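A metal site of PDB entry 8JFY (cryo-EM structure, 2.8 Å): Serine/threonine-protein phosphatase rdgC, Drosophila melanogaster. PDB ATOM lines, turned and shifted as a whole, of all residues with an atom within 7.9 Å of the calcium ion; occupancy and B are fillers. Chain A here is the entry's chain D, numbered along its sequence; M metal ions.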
ATOM      1  N   ILE A  33      18.874   3.853  -5.910  1.00  0.00           N
ATOM      2  CA  ILE A  33      17.528   3.753  -6.486  1.00  0.00           C
ATOM      3  C   ILE A  33      16.476   3.959  -5.402  1.00  0.00           C
ATOM      4  O   ILE A  33      15.419   4.549  -5.658  1.00  0.00           O
ATOM      5  CB  ILE A  33      17.362   2.401  -7.203  1.00  0.00           C
ATOM      6  CG1 ILE A  33      18.106   2.411  -8.537  1.00  0.00           C
ATOM      7  CG2 ILE A  33      15.893   2.071  -7.416  1.00  0.00           C
ATOM      8  CD1 ILE A  33      18.328   1.027  -9.126  1.00  0.00           C
ATOM      9  N   ASN A  36      15.796   7.675  -4.664  1.00  0.00           N
ATOM     10  CA  ASN A  36      15.024   8.295  -5.734  1.00  0.00           C
ATOM     11  C   ASN A  36      13.568   7.860  -5.696  1.00  0.00           C
ATOM     12  O   ASN A  36      12.657   8.667  -5.873  1.00  0.00           O
ATOM     13  CB  ASN A  36      15.647   7.969  -7.097  1.00  0.00           C
ATOM     14  CG  ASN A  36      16.773   8.916  -7.460  1.00  0.00           C
ATOM     15  OD1 ASN A  36      16.544  10.076  -7.813  1.00  0.00           O
ATOM     16  ND2 ASN A  36      18.006   8.438  -7.364  1.00  0.00           N
ATOM     17  N   GLU A 539      15.437  -3.184 -13.863  1.00  0.00           N
ATOM     18  CA  GLU A 539      14.522  -2.074 -14.114  1.00  0.00           C
ATOM     19  C   GLU A 539      13.866  -2.156 -15.497  1.00  0.00           C
ATOM     20  O   GLU A 539      13.798  -1.172 -16.233  1.00  0.00           O
ATOM     21  CB  GLU A 539      15.213  -0.722 -13.895  1.00  0.00           C
ATOM     22  CG  GLU A 539      16.415  -0.418 -14.780  1.00  0.00           C
ATOM     23  CD  GLU A 539      16.944   0.989 -14.597  1.00  0.00           C
ATOM     24  OE1 GLU A 539      16.786   1.544 -13.489  1.00  0.00           O
ATOM     25  OE2 GLU A 539      17.514   1.546 -15.561  1.00  0.00           O
ATOM     26  N   ILE A 540      13.363  -3.352 -15.823  1.00  0.00           N
ATOM     27  CA  ILE A 540      12.565  -3.656 -17.006  1.00  0.00           C
ATOM     28  C   ILE A 540      13.213  -3.107 -18.280  1.00  0.00           C
ATOM     29  O   ILE A 540      14.414  -2.789 -18.289  1.00  0.00           O
ATOM     30  CB  ILE A 540      11.108  -3.156 -16.819  1.00  0.00           C
ATOM     31  CG1 ILE A 540      10.121  -4.007 -17.615  1.00  0.00           C
ATOM     32  CG2 ILE A 540      10.945  -1.659 -17.148  1.00  0.00           C
ATOM     33  CD1 ILE A 540       9.789  -5.327 -16.960  1.00  0.00           C
ATOM     34  N   MET A 572       4.554   4.533 -15.321  1.00  0.00           N
ATOM     35  CA  MET A 572       5.221   3.653 -14.355  1.00  0.00           C
ATOM     36  C   MET A 572       6.643   4.118 -14.060  1.00  0.00           C
ATOM     37  O   MET A 572       7.176   3.815 -12.990  1.00  0.00           O
ATOM     38  CB  MET A 572       5.217   2.207 -14.871  1.00  0.00           C
ATOM     39  CG  MET A 572       3.846   1.569 -14.863  1.00  0.00           C
ATOM     40  SD  MET A 572       2.815   2.178 -13.516  1.00  0.00           S
ATOM     41  CE  MET A 572       1.365   1.140 -13.672  1.00  0.00           C
ATOM     42  N   ASP A 573       7.265   4.835 -14.996  1.00  0.00           N
ATOM     43  CA  ASP A 573       8.574   5.420 -14.732  1.00  0.00           C
ATOM     44  C   ASP A 573       8.403   6.687 -13.908  1.00  0.00           C
ATOM     45  O   ASP A 573       7.661   7.598 -14.300  1.00  0.00           O
ATOM     46  CB  ASP A 573       9.294   5.719 -16.049  1.00  0.00           C
ATOM     47  CG  ASP A 573      10.699   6.259 -15.836  1.00  0.00           C
ATOM     48  OD1 ASP A 573      11.207   6.196 -14.699  1.00  0.00           O
ATOM     49  OD2 ASP A 573      11.299   6.745 -16.822  1.00  0.00           O
ATOM     50  N   LEU A 574       9.094   6.757 -12.770  1.00  0.00           N
ATOM     51  CA  LEU A 574       8.965   7.888 -11.851  1.00  0.00           C
ATOM     52  C   LEU A 574      10.139   8.851 -11.901  1.00  0.00           C
ATOM     53  O   LEU A 574       9.932  10.062 -11.909  1.00  0.00           O
ATOM     54  CB  LEU A 574       8.783   7.376 -10.417  1.00  0.00           C
ATOM     55  CG  LEU A 574       7.550   6.513 -10.148  1.00  0.00           C
ATOM     56  CD1 LEU A 574       7.511   6.046  -8.702  1.00  0.00           C
ATOM     57  CD2 LEU A 574       6.282   7.281 -10.505  1.00  0.00           C
ATOM     58  N   ASN A 575      11.370   8.337 -11.950  1.00  0.00           N
ATOM     59  CA  ASN A 575      12.538   9.206 -11.962  1.00  0.00           C
ATOM     60  C   ASN A 575      12.866   9.754 -13.346  1.00  0.00           C
ATOM     61  O   ASN A 575      13.694  10.667 -13.455  1.00  0.00           O
ATOM     62  CB  ASN A 575      13.758   8.460 -11.408  1.00  0.00           C
ATOM     63  CG  ASN A 575      14.062   7.177 -12.143  1.00  0.00           C
ATOM     64  OD1 ASN A 575      13.484   6.905 -13.200  1.00  0.00           O
ATOM     65  ND2 ASN A 575      14.968   6.380 -11.599  1.00  0.00           N
ATOM     66  N   GLY A 576      12.239   9.233 -14.394  1.00  0.00           N
ATOM     67  CA  GLY A 576      12.408   9.769 -15.737  1.00  0.00           C
ATOM     68  C   GLY A 576      13.592   9.243 -16.513  1.00  0.00           C
ATOM     69  O   GLY A 576      13.984   9.868 -17.507  1.00  0.00           O
ATOM     70  N   ASP A 577      14.174   8.114 -16.106  1.00  0.00           N
ATOM     71  CA  ASP A 577      15.312   7.564 -16.833  1.00  0.00           C
ATOM     72  C   ASP A 577      14.896   6.701 -18.021  1.00  0.00           C
ATOM     73  O   ASP A 577      15.782   6.183 -18.720  1.00  0.00           O
ATOM     74  CB  ASP A 577      16.211   6.754 -15.887  1.00  0.00           C
ATOM     75  CG  ASP A 577      15.451   5.674 -15.133  1.00  0.00           C
ATOM     76  OD1 ASP A 577      14.302   5.368 -15.499  1.00  0.00           O
ATOM     77  OD2 ASP A 577      16.012   5.130 -14.160  1.00  0.00           O
ATOM     78  N   GLY A 578      13.601   6.527 -18.247  1.00  0.00           N
ATOM     79  CA  GLY A 578      13.118   5.683 -19.331  1.00  0.00           C
ATOM     80  C   GLY A 578      12.940   4.225 -18.974  1.00  0.00           C
ATOM     81  O   GLY A 578      12.557   3.438 -19.843  1.00  0.00           O
ATOM     82  N   LYS A 579      13.219   3.841 -17.729  1.00  0.00           N
ATOM     83  CA  LYS A 579      13.081   2.462 -17.281  1.00  0.00           C
ATOM     84  C   LYS A 579      12.292   2.435 -15.990  1.00  0.00           C
ATOM     85  O   LYS A 579      12.228   3.423 -15.249  1.00  0.00           O
ATOM     86  CB  LYS A 579      14.464   1.797 -17.102  1.00  0.00           C
ATOM     87  CG  LYS A 579      15.006   1.160 -18.367  1.00  0.00           C
ATOM     88  CD  LYS A 579      15.746   2.164 -19.234  1.00  0.00           C
ATOM     89  CE  LYS A 579      17.077   2.562 -18.618  1.00  0.00           C
ATOM     90  NZ  LYS A 579      17.726   3.672 -19.366  1.00  0.00           N
ATOM     91  N   VAL A 580      11.683   1.290 -15.701  1.00  0.00           N
ATOM     92  CA  VAL A 580      10.828   1.145 -14.520  1.00  0.00           C
ATOM     93  C   VAL A 580      11.356   0.029 -13.638  1.00  0.00           C
ATOM     94  O   VAL A 580      11.304  -1.155 -14.006  1.00  0.00           O
ATOM     95  CB  VAL A 580       9.367   0.887 -14.922  1.00  0.00           C
ATOM     96  CG1 VAL A 580       8.485   0.828 -13.694  1.00  0.00           C
ATOM     97  CG2 VAL A 580       8.882   1.958 -15.892  1.00  0.00           C
ATOM     98  N   ASP A 581      11.851   0.386 -12.458  1.00  0.00           N
ATOM     99  CA  ASP A 581      12.286  -0.613 -11.495  1.00  0.00           C
ATOM    100  C   ASP A 581      11.078  -1.328 -10.897  1.00  0.00           C
ATOM    101  O   ASP A 581       9.956  -0.835 -10.925  1.00  0.00           O
ATOM    102  CB  ASP A 581      13.128   0.040 -10.397  1.00  0.00           C
ATOM    103  CG  ASP A 581      13.728  -0.968  -9.440  1.00  0.00           C
ATOM    104  OD1 ASP A 581      14.344  -1.951  -9.910  1.00  0.00           O
ATOM    105  OD2 ASP A 581      13.589  -0.782  -8.204  1.00  0.00           O
ATOM    106  N   GLU A 584       9.923   0.739  -8.252  1.00  0.00           N
ATOM    107  CA  GLU A 584       9.300   1.905  -8.874  1.00  0.00           C
ATOM    108  C   GLU A 584       7.873   1.597  -9.323  1.00  0.00           C
ATOM    109  O   GLU A 584       6.949   2.400  -9.095  1.00  0.00           O
ATOM    110  CB  GLU A 584      10.138   2.382 -10.057  1.00  0.00           C
ATOM    111  CG  GLU A 584      10.075   3.869 -10.325  1.00  0.00           C
ATOM    112  CD  GLU A 584      11.232   4.358 -11.178  1.00  0.00           C
ATOM    113  OE1 GLU A 584      11.879   3.524 -11.839  1.00  0.00           O
ATOM    114  OE2 GLU A 584      11.485   5.583 -11.188  1.00  0.00           O
ATOM    115  N   PHE A 585       7.676   0.445  -9.962  1.00  0.00           N
ATOM    116  CA  PHE A 585       6.343   0.010 -10.380  1.00  0.00           C
ATOM    117  C   PHE A 585       5.431  -0.158  -9.169  1.00  0.00           C
ATOM    118  O   PHE A 585       4.272   0.293  -9.185  1.00  0.00           O
ATOM    119  CB  PHE A 585       6.471  -1.287 -11.168  1.00  0.00           C
ATOM    120  CG  PHE A 585       5.168  -1.838 -11.682  1.00  0.00           C
ATOM    121  CD1 PHE A 585       4.433  -1.160 -12.635  1.00  0.00           C
ATOM    122  CD2 PHE A 585       4.702  -3.056 -11.217  1.00  0.00           C
ATOM    123  CE1 PHE A 585       3.247  -1.686 -13.110  1.00  0.00           C
ATOM    124  CE2 PHE A 585       3.517  -3.581 -11.692  1.00  0.00           C
ATOM    125  CZ  PHE A 585       2.788  -2.893 -12.632  1.00  0.00           C
HETATM  126 CA    CA M   1      13.249   4.581 -13.447  1.00  0.00          CA
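The side-chain carboxylate of Asp 573 lies close to the backbone NH of Gly 576 (3.2 Å). The side-chain carboxylate (OD2) of Asp 573 lies within hydrogen-bond range of the backbone NH (N) of Gly 578. The side-chain carboxylate (OE1) of Glu 584 sits close to the backbone NH (N) of Asp 581 (3.2 Å). OE2 of Glu 584 sits at hydrogen-bond distance from N of Leu 574.
Five residues have an atom within 4 Å of the calcium ion: Asp 573, Asn 575, Asp 577, Lys 579 and Glu 584. The nearest printed residue that does not touch the calcium ion is Val 580 (4.3 Å).
The calcium ion is bound by OD1 of Asn 575 (2.3 Å), OE1 of Glu 584 (2.4 Å), O of Lys 579 (2.4 Å), OD1 of Asp 577 (2.4 Å) and OD1 of Asp 573 (2.9 Å). The calcium ion has five donor atoms within binding distance. Slightly farther from the calcium ion lies the side-chain carboxylate (OD2) of Asp 577 (2.9 Å). Slightly farther from the calcium ion lies the side-chain carboxylate (OE2) of Glu 584 (3.0 Å). Slightly farther from the calcium ion lies ND2 of Asn 575 (3.1 Å).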
